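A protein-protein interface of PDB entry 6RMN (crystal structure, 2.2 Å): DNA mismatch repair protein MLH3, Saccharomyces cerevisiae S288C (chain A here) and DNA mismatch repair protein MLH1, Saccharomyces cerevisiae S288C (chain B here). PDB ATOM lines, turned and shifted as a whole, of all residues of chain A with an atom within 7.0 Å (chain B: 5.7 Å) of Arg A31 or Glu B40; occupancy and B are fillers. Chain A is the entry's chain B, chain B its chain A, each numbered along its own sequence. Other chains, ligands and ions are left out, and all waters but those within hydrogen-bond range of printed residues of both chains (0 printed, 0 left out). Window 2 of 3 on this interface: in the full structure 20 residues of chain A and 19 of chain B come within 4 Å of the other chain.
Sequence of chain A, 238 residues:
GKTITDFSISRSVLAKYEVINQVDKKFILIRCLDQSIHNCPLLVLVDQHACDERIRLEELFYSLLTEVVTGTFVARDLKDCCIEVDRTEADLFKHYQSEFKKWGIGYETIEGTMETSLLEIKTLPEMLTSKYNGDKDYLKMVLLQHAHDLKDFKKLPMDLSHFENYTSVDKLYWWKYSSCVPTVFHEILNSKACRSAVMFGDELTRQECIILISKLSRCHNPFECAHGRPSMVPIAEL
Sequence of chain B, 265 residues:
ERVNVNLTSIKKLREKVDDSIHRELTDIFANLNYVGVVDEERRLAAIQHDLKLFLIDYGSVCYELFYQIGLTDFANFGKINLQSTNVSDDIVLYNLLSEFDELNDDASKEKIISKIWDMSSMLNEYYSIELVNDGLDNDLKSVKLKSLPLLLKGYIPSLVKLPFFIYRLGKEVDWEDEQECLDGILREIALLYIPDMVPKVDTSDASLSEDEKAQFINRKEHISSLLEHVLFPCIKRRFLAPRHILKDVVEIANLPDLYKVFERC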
ATOM      1  N   LEU A  14      22.194 -26.421 -26.080  1.00  0.00           N
ATOM      2  CA  LEU A  14      22.405 -25.355 -27.065  1.00  0.00           C
ATOM      3  C   LEU A  14      21.137 -24.593 -27.437  1.00  0.00           C
ATOM      4  O   LEU A  14      21.225 -23.406 -27.771  1.00  0.00           O
ATOM      5  CB  LEU A  14      23.033 -25.914 -28.351  1.00  0.00           C
ATOM      6  CG  LEU A  14      24.438 -25.445 -28.744  1.00  0.00           C
ATOM      7  CD1 LEU A  14      24.710 -25.763 -30.193  1.00  0.00           C
ATOM      8  CD2 LEU A  14      24.629 -23.952 -28.533  1.00  0.00           C
ATOM      9  N   LYS A  16      18.726 -23.651 -25.491  1.00  0.00           N
ATOM     10  CA  LYS A  16      18.492 -22.664 -24.429  1.00  0.00           C
ATOM     11  C   LYS A  16      19.568 -21.545 -24.413  1.00  0.00           C
ATOM     12  O   LYS A  16      19.689 -20.857 -23.406  1.00  0.00           O
ATOM     13  CB  LYS A  16      18.506 -23.377 -23.061  1.00  0.00           C
ATOM     14  CG  LYS A  16      17.346 -24.326 -22.785  1.00  0.00           C
ATOM     15  CD  LYS A  16      17.724 -25.298 -21.662  1.00  0.00           C
ATOM     16  CE  LYS A  16      16.536 -25.840 -20.900  1.00  0.00           C
ATOM     17  NZ  LYS A  16      16.077 -24.905 -19.835  1.00  0.00           N
ATOM     18  N   TYR A  17      20.351 -21.371 -25.503  1.00  0.00           N
ATOM     19  CA  TYR A  17      21.451 -20.407 -25.547  1.00  0.00           C
ATOM     20  C   TYR A  17      21.274 -19.217 -26.482  1.00  0.00           C
ATOM     21  O   TYR A  17      21.265 -19.396 -27.710  1.00  0.00           O
ATOM     22  CB  TYR A  17      22.788 -21.107 -25.876  1.00  0.00           C
ATOM     23  CG  TYR A  17      23.479 -21.722 -24.677  1.00  0.00           C
ATOM     24  CD1 TYR A  17      23.095 -22.965 -24.189  1.00  0.00           C
ATOM     25  CD2 TYR A  17      24.535 -21.072 -24.046  1.00  0.00           C
ATOM     26  CE1 TYR A  17      23.713 -23.529 -23.077  1.00  0.00           C
ATOM     27  CE2 TYR A  17      25.174 -21.633 -22.945  1.00  0.00           C
ATOM     28  CZ  TYR A  17      24.753 -22.858 -22.456  1.00  0.00           C
ATOM     29  OH  TYR A  17      25.349 -23.417 -21.350  1.00  0.00           O
ATOM     30  N   GLU A  18      21.257 -17.989 -25.883  1.00  0.00           N
ATOM     31  CA  GLU A  18      21.197 -16.678 -26.544  1.00  0.00           C
ATOM     32  C   GLU A  18      22.619 -16.106 -26.780  1.00  0.00           C
ATOM     33  O   GLU A  18      23.481 -16.204 -25.905  1.00  0.00           O
ATOM     34  CB  GLU A  18      20.360 -15.688 -25.700  1.00  0.00           C
ATOM     35  CG  GLU A  18      19.964 -14.424 -26.451  1.00  0.00           C
ATOM     36  CD  GLU A  18      18.970 -13.501 -25.774  1.00  0.00           C
ATOM     37  OE1 GLU A  18      17.793 -13.899 -25.612  1.00  0.00           O
ATOM     38  OE2 GLU A  18      19.362 -12.360 -25.437  1.00  0.00           O
ATOM     39  N   VAL A  19      22.845 -15.482 -27.950  1.00  0.00           N
ATOM     40  CA  VAL A  19      24.132 -14.869 -28.325  1.00  0.00           C
ATOM     41  C   VAL A  19      24.351 -13.522 -27.626  1.00  0.00           C
ATOM     42  O   VAL A  19      23.492 -12.644 -27.690  1.00  0.00           O
ATOM     43  CB  VAL A  19      24.292 -14.694 -29.876  1.00  0.00           C
ATOM     44  CG1 VAL A  19      25.597 -13.979 -30.235  1.00  0.00           C
ATOM     45  CG2 VAL A  19      24.206 -16.026 -30.613  1.00  0.00           C
ATOM     46  N   ILE A  20      25.554 -13.328 -27.074  1.00  0.00           N
ATOM     47  CA  ILE A  20      25.977 -12.060 -26.508  1.00  0.00           C
ATOM     48  C   ILE A  20      26.643 -11.308 -27.682  1.00  0.00           C
ATOM     49  O   ILE A  20      25.992 -10.448 -28.275  1.00  0.00           O
ATOM     50  CB  ILE A  20      26.840 -12.232 -25.219  1.00  0.00           C
ATOM     51  CG1 ILE A  20      26.019 -13.007 -24.142  1.00  0.00           C
ATOM     52  CG2 ILE A  20      27.329 -10.855 -24.687  1.00  0.00           C
ATOM     53  CD1 ILE A  20      26.702 -13.315 -22.885  1.00  0.00           C
ATOM     54  N   LEU A  29      30.515 -15.443 -28.017  1.00  0.00           N
ATOM     55  CA  LEU A  29      30.122 -15.618 -26.623  1.00  0.00           C
ATOM     56  C   LEU A  29      28.615 -15.836 -26.549  1.00  0.00           C
ATOM     57  O   LEU A  29      27.836 -15.047 -27.097  1.00  0.00           O
ATOM     58  CB  LEU A  29      30.560 -14.428 -25.745  1.00  0.00           C
ATOM     59  CG  LEU A  29      30.209 -14.476 -24.227  1.00  0.00           C
ATOM     60  CD1 LEU A  29      30.986 -15.591 -23.486  1.00  0.00           C
ATOM     61  CD2 LEU A  29      30.473 -13.109 -23.563  1.00  0.00           C
ATOM     62  N   ILE A  30      28.219 -16.947 -25.905  1.00  0.00           N
ATOM     63  CA  ILE A  30      26.820 -17.331 -25.732  1.00  0.00           C
ATOM     64  C   ILE A  30      26.485 -17.548 -24.250  1.00  0.00           C
ATOM     65  O   ILE A  30      27.355 -17.917 -23.452  1.00  0.00           O
ATOM     66  CB  ILE A  30      26.413 -18.530 -26.648  1.00  0.00           C
ATOM     67  CG1 ILE A  30      27.162 -19.846 -26.284  1.00  0.00           C
ATOM     68  CG2 ILE A  30      26.583 -18.175 -28.153  1.00  0.00           C
ATOM     69  CD1 ILE A  30      26.577 -21.185 -26.906  1.00  0.00           C
ATOM     70  N   ARG A  31      25.232 -17.262 -23.879  1.00  0.00           N
ATOM     71  CA  ARG A  31      24.730 -17.445 -22.513  1.00  0.00           C
ATOM     72  C   ARG A  31      23.515 -18.355 -22.506  1.00  0.00           C
ATOM     73  O   ARG A  31      22.715 -18.303 -23.440  1.00  0.00           O
ATOM     74  CB  ARG A  31      24.380 -16.101 -21.834  1.00  0.00           C
ATOM     75  CG  ARG A  31      23.341 -15.231 -22.575  1.00  0.00           C
ATOM     76  CD  ARG A  31      23.004 -13.970 -21.810  1.00  0.00           C
ATOM     77  NE  ARG A  31      22.061 -13.120 -22.537  1.00  0.00           N
ATOM     78  CZ  ARG A  31      21.288 -12.195 -21.976  1.00  0.00           C
ATOM     79  NH1 ARG A  31      21.319 -11.998 -20.663  1.00  0.00           N
ATOM     80  NH2 ARG A  31      20.464 -11.472 -22.720  1.00  0.00           N
ATOM     81  N   CYS A  32      23.366 -19.176 -21.452  1.00  0.00           N
ATOM     82  CA  CYS A  32      22.197 -20.044 -21.273  1.00  0.00           C
ATOM     83  C   CYS A  32      20.971 -19.205 -20.853  1.00  0.00           C
ATOM     84  O   CYS A  32      21.078 -18.282 -20.038  1.00  0.00           O
ATOM     85  CB  CYS A  32      22.482 -21.158 -20.271  1.00  0.00           C
ATOM     86  SG  CYS A  32      21.080 -22.272 -19.982  1.00  0.00           S
ATOM     87  N   LEU A  42      26.541 -21.848 -17.996  1.00  0.00           N
ATOM     88  CA  LEU A  42      25.966 -20.511 -18.190  1.00  0.00           C
ATOM     89  C   LEU A  42      26.636 -19.733 -19.342  1.00  0.00           C
ATOM     90  O   LEU A  42      25.922 -19.260 -20.219  1.00  0.00           O
ATOM     91  CB  LEU A  42      25.942 -19.680 -16.880  1.00  0.00           C
ATOM     92  CG  LEU A  42      25.431 -18.201 -16.990  1.00  0.00           C
ATOM     93  CD1 LEU A  42      23.962 -18.077 -16.586  1.00  0.00           C
ATOM     94  CD2 LEU A  42      26.296 -17.237 -16.166  1.00  0.00           C
ATOM     95  N   LEU A  43      27.976 -19.572 -19.328  1.00  0.00           N
ATOM     96  CA  LEU A  43      28.713 -18.855 -20.380  1.00  0.00           C
ATOM     97  C   LEU A  43      29.595 -19.798 -21.192  1.00  0.00           C
ATOM     98  O   LEU A  43      30.375 -20.569 -20.624  1.00  0.00           O
ATOM     99  CB  LEU A  43      29.549 -17.672 -19.831  1.00  0.00           C
ATOM    100  CG  LEU A  43      28.828 -16.378 -19.380  1.00  0.00           C
ATOM    101  CD1 LEU A  43      29.837 -15.306 -19.016  1.00  0.00           C
ATOM    102  CD2 LEU A  43      27.908 -15.808 -20.458  1.00  0.00           C
ATOM    103  N   VAL A  44      29.463 -19.738 -22.525  1.00  0.00           N
ATOM    104  CA  VAL A  44      30.209 -20.578 -23.465  1.00  0.00           C
ATOM    105  C   VAL A  44      30.815 -19.722 -24.600  1.00  0.00           C
ATOM    106  O   VAL A  44      30.153 -18.810 -25.116  1.00  0.00           O
ATOM    107  CB  VAL A  44      29.300 -21.731 -24.014  1.00  0.00           C
ATOM    108  CG1 VAL A  44      29.927 -22.464 -25.204  1.00  0.00           C
ATOM    109  CG2 VAL A  44      28.914 -22.722 -22.917  1.00  0.00           C
ATOM    110  N   ARG A 206      26.659  -9.007 -34.777  1.00  0.00           N
ATOM    111  CA  ARG A 206      25.874  -9.825 -33.830  1.00  0.00           C
ATOM    112  C   ARG A 206      24.829 -10.672 -34.597  1.00  0.00           C
ATOM    113  O   ARG A 206      24.637 -11.833 -34.269  1.00  0.00           O
ATOM    114  CB  ARG A 206      25.197  -8.950 -32.739  1.00  0.00           C
ATOM    115  CG  ARG A 206      24.848  -9.742 -31.474  1.00  0.00           C
ATOM    116  CD  ARG A 206      24.199  -8.892 -30.405  1.00  0.00           C
ATOM    117  NE  ARG A 206      22.745  -8.888 -30.548  1.00  0.00           N
ATOM    118  CZ  ARG A 206      21.909  -9.594 -29.791  1.00  0.00           C
ATOM    119  NH1 ARG A 206      22.371 -10.350 -28.804  1.00  0.00           N
ATOM    120  NH2 ARG A 206      20.600  -9.539 -30.010  1.00  0.00           N
ATOM    121  N   VAL B  37      25.752  -7.468 -22.750  1.00  0.00           N
ATOM    122  CA  VAL B  37      25.023  -7.812 -21.521  1.00  0.00           C
ATOM    123  C   VAL B  37      24.991  -9.334 -21.339  1.00  0.00           C
ATOM    124  O   VAL B  37      24.575 -10.060 -22.248  1.00  0.00           O
ATOM    125  CB  VAL B  37      23.585  -7.207 -21.443  1.00  0.00           C
ATOM    126  CG1 VAL B  37      22.897  -7.549 -20.119  1.00  0.00           C
ATOM    127  CG2 VAL B  37      23.592  -5.701 -21.654  1.00  0.00           C
ATOM    128  N   VAL B  38      25.373  -9.782 -20.117  1.00  0.00           N
ATOM    129  CA  VAL B  38      25.390 -11.157 -19.644  1.00  0.00           C
ATOM    130  C   VAL B  38      24.105 -11.466 -18.838  1.00  0.00           C
ATOM    131  O   VAL B  38      23.534 -12.531 -19.030  1.00  0.00           O
ATOM    132  CB  VAL B  38      26.698 -11.448 -18.851  1.00  0.00           C
ATOM    133  CG1 VAL B  38      26.635 -12.789 -18.113  1.00  0.00           C
ATOM    134  CG2 VAL B  38      27.923 -11.386 -19.772  1.00  0.00           C
ATOM    135  N   ASP B  39      23.661 -10.556 -17.940  1.00  0.00           N
ATOM    136  CA  ASP B  39      22.458 -10.742 -17.104  1.00  0.00           C
ATOM    137  C   ASP B  39      21.855  -9.378 -16.780  1.00  0.00           C
ATOM    138  O   ASP B  39      22.509  -8.574 -16.128  1.00  0.00           O
ATOM    139  CB  ASP B  39      22.819 -11.514 -15.804  1.00  0.00           C
ATOM    140  CG  ASP B  39      21.681 -11.953 -14.875  1.00  0.00           C
ATOM    141  OD1 ASP B  39      20.590 -11.320 -14.908  1.00  0.00           O
ATOM    142  OD2 ASP B  39      21.889 -12.911 -14.094  1.00  0.00           O
ATOM    143  N   GLU B  40      20.607  -9.128 -17.220  1.00  0.00           N
ATOM    144  CA  GLU B  40      19.872  -7.865 -17.033  1.00  0.00           C
ATOM    145  C   GLU B  40      19.265  -7.691 -15.640  1.00  0.00           C
ATOM    146  O   GLU B  40      18.951  -6.567 -15.244  1.00  0.00           O
ATOM    147  CB  GLU B  40      18.755  -7.713 -18.082  1.00  0.00           C
ATOM    148  CG  GLU B  40      19.215  -7.545 -19.519  1.00  0.00           C
ATOM    149  CD  GLU B  40      19.456  -8.823 -20.304  1.00  0.00           C
ATOM    150  OE1 GLU B  40      19.692  -8.718 -21.529  1.00  0.00           O
ATOM    151  OE2 GLU B  40      19.408  -9.925 -19.707  1.00  0.00           O
ATOM    152  N   GLU B  41      19.049  -8.800 -14.928  1.00  0.00           N
ATOM    153  CA  GLU B  41      18.471  -8.809 -13.591  1.00  0.00           C
ATOM    154  C   GLU B  41      19.551  -8.523 -12.537  1.00  0.00           C
ATOM    155  O   GLU B  41      19.335  -7.686 -11.659  1.00  0.00           O
ATOM    156  CB  GLU B  41      17.754 -10.143 -13.331  1.00  0.00           C
ATOM    157  CG  GLU B  41      16.803 -10.105 -12.145  1.00  0.00           C
ATOM    158  CD  GLU B  41      15.903 -11.314 -11.957  1.00  0.00           C
ATOM    159  OE1 GLU B  41      15.126 -11.317 -10.975  1.00  0.00           O
ATOM    160  OE2 GLU B  41      15.971 -12.257 -12.780  1.00  0.00           O
ATOM    161  N   ARG B  42      20.704  -9.205 -12.631  1.00  0.00           N
ATOM    162  CA  ARG B  42      21.839  -9.025 -11.726  1.00  0.00           C
ATOM    163  C   ARG B  42      22.791  -7.920 -12.219  1.00  0.00           C
ATOM    164  O   ARG B  42      23.816  -7.652 -11.576  1.00  0.00           O
ATOM    165  CB  ARG B  42      22.593 -10.350 -11.527  1.00  0.00           C
ATOM    166  CG  ARG B  42      21.995 -11.240 -10.440  1.00  0.00           C
ATOM    167  CD  ARG B  42      22.913 -12.392 -10.056  1.00  0.00           C
ATOM    168  NE  ARG B  42      23.220 -13.269 -11.188  1.00  0.00           N
ATOM    169  CZ  ARG B  42      24.395 -13.864 -11.383  1.00  0.00           C
ATOM    170  NH1 ARG B  42      25.389 -13.688 -10.518  1.00  0.00           N
ATOM    171  NH2 ARG B  42      24.587 -14.636 -12.447  1.00  0.00           N
ATOM    172  N   ARG B  43      22.433  -7.267 -13.351  1.00  0.00           N
ATOM    173  CA  ARG B  43      23.166  -6.178 -14.005  1.00  0.00           C
ATOM    174  C   ARG B  43      24.637  -6.529 -14.264  1.00  0.00           C
ATOM    175  O   ARG B  43      25.540  -5.825 -13.802  1.00  0.00           O
ATOM    176  CB  ARG B  43      23.009  -4.841 -13.268  1.00  0.00           C
ATOM    177  CG  ARG B  43      21.637  -4.210 -13.439  1.00  0.00           C
ATOM    178  CD  ARG B  43      21.559  -2.846 -12.777  1.00  0.00           C
ATOM    179  NE  ARG B  43      21.534  -2.932 -11.312  1.00  0.00           N
ATOM    180  CZ  ARG B  43      20.771  -2.177 -10.526  1.00  0.00           C
ATOM    181  NH1 ARG B  43      19.934  -1.296 -11.052  1.00  0.00           N
ATOM    182  NH2 ARG B  43      20.803  -2.335  -9.210  1.00  0.00           N
ATOM    183  N   LEU B  44      24.859  -7.608 -15.048  1.00  0.00           N
ATOM    184  CA  LEU B  44      26.178  -8.086 -15.435  1.00  0.00           C
ATOM    185  C   LEU B  44      26.423  -7.896 -16.933  1.00  0.00           C
ATOM    186  O   LEU B  44      25.515  -8.104 -17.739  1.00  0.00           O
ATOM    187  CB  LEU B  44      26.388  -9.564 -15.044  1.00  0.00           C
ATOM    188  CG  LEU B  44      26.135  -9.959 -13.564  1.00  0.00           C
ATOM    189  CD1 LEU B  44      26.277 -11.462 -13.366  1.00  0.00           C
ATOM    190  CD2 LEU B  44      27.051  -9.208 -12.610  1.00  0.00           C
ATOM    191  N   TYR B  58      27.578  -3.708 -13.841  1.00  0.00           N
ATOM    192  CA  TYR B  58      27.407  -2.339 -14.354  1.00  0.00           C
ATOM    193  C   TYR B  58      26.485  -1.482 -13.487  1.00  0.00           C
ATOM    194  O   TYR B  58      26.471  -0.265 -13.663  1.00  0.00           O
ATOM    195  CB  TYR B  58      27.009  -2.272 -15.847  1.00  0.00           C
ATOM    196  CG  TYR B  58      25.677  -2.903 -16.194  1.00  0.00           C
ATOM    197  CD1 TYR B  58      24.491  -2.180 -16.088  1.00  0.00           C
ATOM    198  CD2 TYR B  58      25.608  -4.202 -16.680  1.00  0.00           C
ATOM    199  CE1 TYR B  58      23.267  -2.747 -16.439  1.00  0.00           C
ATOM    200  CE2 TYR B  58      24.393  -4.776 -17.038  1.00  0.00           C
ATOM    201  CZ  TYR B  58      23.224  -4.052 -16.904  1.00  0.00           C
ATOM    202  OH  TYR B  58      22.032  -4.648 -17.220  1.00  0.00           O
ATOM    203  N   ASP B 196      17.951   0.604 -14.713  1.00  0.00           N
ATOM    204  CA  ASP B 196      17.070  -0.324 -13.995  1.00  0.00           C
ATOM    205  C   ASP B 196      17.456  -1.776 -14.198  1.00  0.00           C
ATOM    206  O   ASP B 196      18.098  -2.123 -15.198  1.00  0.00           O
ATOM    207  CB  ASP B 196      15.606  -0.163 -14.464  1.00  0.00           C
ATOM    208  CG  ASP B 196      14.881   1.126 -14.126  1.00  0.00           C
ATOM    209  OD1 ASP B 196      15.196   1.735 -13.079  1.00  0.00           O
ATOM    210  OD2 ASP B 196      13.969   1.501 -14.884  1.00  0.00           O
ATOM    211  N   MET B 197      17.032  -2.630 -13.260  1.00  0.00           N
ATOM    212  CA  MET B 197      17.208  -4.072 -13.336  1.00  0.00           C
ATOM    213  C   MET B 197      16.034  -4.588 -14.157  1.00  0.00           C
ATOM    214  O   MET B 197      14.935  -4.032 -14.066  1.00  0.00           O
ATOM    215  CB  MET B 197      17.132  -4.703 -11.946  1.00  0.00           C
ATOM    216  CG  MET B 197      18.351  -4.486 -11.118  1.00  0.00           C
ATOM    217  SD  MET B 197      18.151  -5.107  -9.426  1.00  0.00           S
ATOM    218  CE  MET B 197      17.193  -3.759  -8.670  1.00  0.00           C
ATOM    219  N   VAL B 198      16.256  -5.639 -14.956  1.00  0.00           N
ATOM    220  CA  VAL B 198      15.186  -6.234 -15.760  1.00  0.00           C
ATOM    221  C   VAL B 198      14.899  -7.644 -15.232  1.00  0.00           C
ATOM    222  O   VAL B 198      15.638  -8.580 -15.563  1.00  0.00           O
ATOM    223  CB  VAL B 198      15.408  -6.156 -17.303  1.00  0.00           C
ATOM    224  CG1 VAL B 198      14.199  -6.700 -18.066  1.00  0.00           C
ATOM    225  CG2 VAL B 198      15.708  -4.722 -17.747  1.00  0.00           C
ATOM    226  N   PRO B 199      13.861  -7.799 -14.362  1.00  0.00           N
ATOM    227  CA  PRO B 199      13.545  -9.137 -13.816  1.00  0.00           C
ATOM    228  C   PRO B 199      13.266 -10.168 -14.909  1.00  0.00           C
ATOM    229  O   PRO B 199      12.598  -9.837 -15.891  1.00  0.00           O
ATOM    230  CB  PRO B 199      12.318  -8.884 -12.928  1.00  0.00           C
ATOM    231  CG  PRO B 199      12.359  -7.430 -12.622  1.00  0.00           C
ATOM    232  CD  PRO B 199      12.913  -6.786 -13.855  1.00  0.00           C
ATOM    233  N   LYS B 220      15.010  -5.364 -22.644  1.00  0.00           N
ATOM    234  CA  LYS B 220      16.328  -5.978 -22.836  1.00  0.00           C
ATOM    235  C   LYS B 220      17.096  -5.226 -23.930  1.00  0.00           C
ATOM    236  O   LYS B 220      18.286  -4.952 -23.771  1.00  0.00           O
ATOM    237  CB  LYS B 220      16.180  -7.458 -23.231  1.00  0.00           C
ATOM    238  CG  LYS B 220      15.853  -8.407 -22.079  1.00  0.00           C
ATOM    239  CD  LYS B 220      15.514  -9.833 -22.572  1.00  0.00           C
ATOM    240  CE  LYS B 220      16.718 -10.727 -22.785  1.00  0.00           C
ATOM    241  NZ  LYS B 220      16.324 -12.152 -22.979  1.00  0.00           N
ATOM    242  N   ILE B 223      18.249  -1.521 -22.648  1.00  0.00           N
ATOM    243  CA  ILE B 223      19.439  -1.512 -21.797  1.00  0.00           C
ATOM    244  C   ILE B 223      20.711  -1.782 -22.649  1.00  0.00           C
ATOM    245  O   ILE B 223      21.681  -1.025 -22.550  1.00  0.00           O
ATOM    246  CB  ILE B 223      19.319  -2.410 -20.514  1.00  0.00           C
ATOM    247  CG1 ILE B 223      20.639  -2.473 -19.718  1.00  0.00           C
ATOM    248  CG2 ILE B 223      18.820  -3.815 -20.796  1.00  0.00           C
ATOM    249  CD1 ILE B 223      21.057  -1.162 -19.066  1.00  0.00           C
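The backbone carbonyl oxygen (O) of Val B38 sits at hydrogen-bond distance from the guanidinium group (NH1) of Arg A31, at 2.8 Å. OE2 of Glu B40 is in salt-bridge range of NH1 of Arg A31, at 3.0 Å. The side-chain amino group of Lys B220 is in salt-bridge range of the side-chain carboxylate of Glu A18, at 3.5 Å.
OD1 of Asp B39 lies within hydrogen-bond range of N of Glu B41, 3.0 Å away. The side-chain carboxylate of Asp B39 lies within salt-bridge range of the guanidinium group of Arg B42, at 3.2 Å. The backbone carbonyl oxygen (O) of Asp B39 sits at hydrogen-bond distance from the backbone NH (N) of Leu B44, at 2.8 Å. O of Glu B40 lies within hydrogen-bond range of N of Val B198. The side-chain carboxylate (OE2) of Glu A18 is in salt-bridge range of the guanidinium group (NH2) of Arg A31 (3.1 Å). O of Leu A29 is in hydrogen-bond range of N of Ile A20.
Among the printed residues, merely in contact across the chains: Ile A20 with Val B37, Ile A20 with Val B38, Arg A31 with Val B37, Arg A31 with Asp B39 and Arg A31 with Lys B220.
Of the printed residues of chain B, Glu A18 touches Lys B220. Printed residues of chain B within 4 Å of Ile A20: Val B37 (3.8 Å) and Val B38 (3.9 Å). Arg A31 touches just these residues of chain B: Val B37 (3.9 Å), Val B38 (2.8 Å), Asp B39 (3.9 Å), Glu B40 (3.0 Å) and Lys B220 (3.8 Å). Of the printed residues of chain A, Val B37 touches Ile A20 (3.8 Å) and Arg A31 (3.9 Å). Printed residues of chain A within 4 Å of Val B38: Ile A20 and Arg A31. Of chain A, only Arg A31 (3.0 Å) comes within 4 Å of Glu B40. The nearest printed residue of chain A that does not touch Asp B39 is Leu A42 (6.1 Å).
Of the 15 printed residues of chain B, 5 touch a printed residue of chain A. Hydrophobic or aromatic side chains of chain B within 4 Å of the printed part of chain A: Val B38. Of the 14 printed residues of chain A, 3 touch a printed residue of chain B. Hydrophobic or aromatic side chains of chain A within 4 Å of the printed part of chain B: Ile A20. Among the printed residues, 8 pairs touch across the chains. Among the printed residues, Asp or Glu carboxylates within 4 Å of a Lys or Arg side-chain nitrogen of the other chain: Glu A18 with Lys B220 (3.5 Å) and Arg A31 with Glu B40 (3.0 Å).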
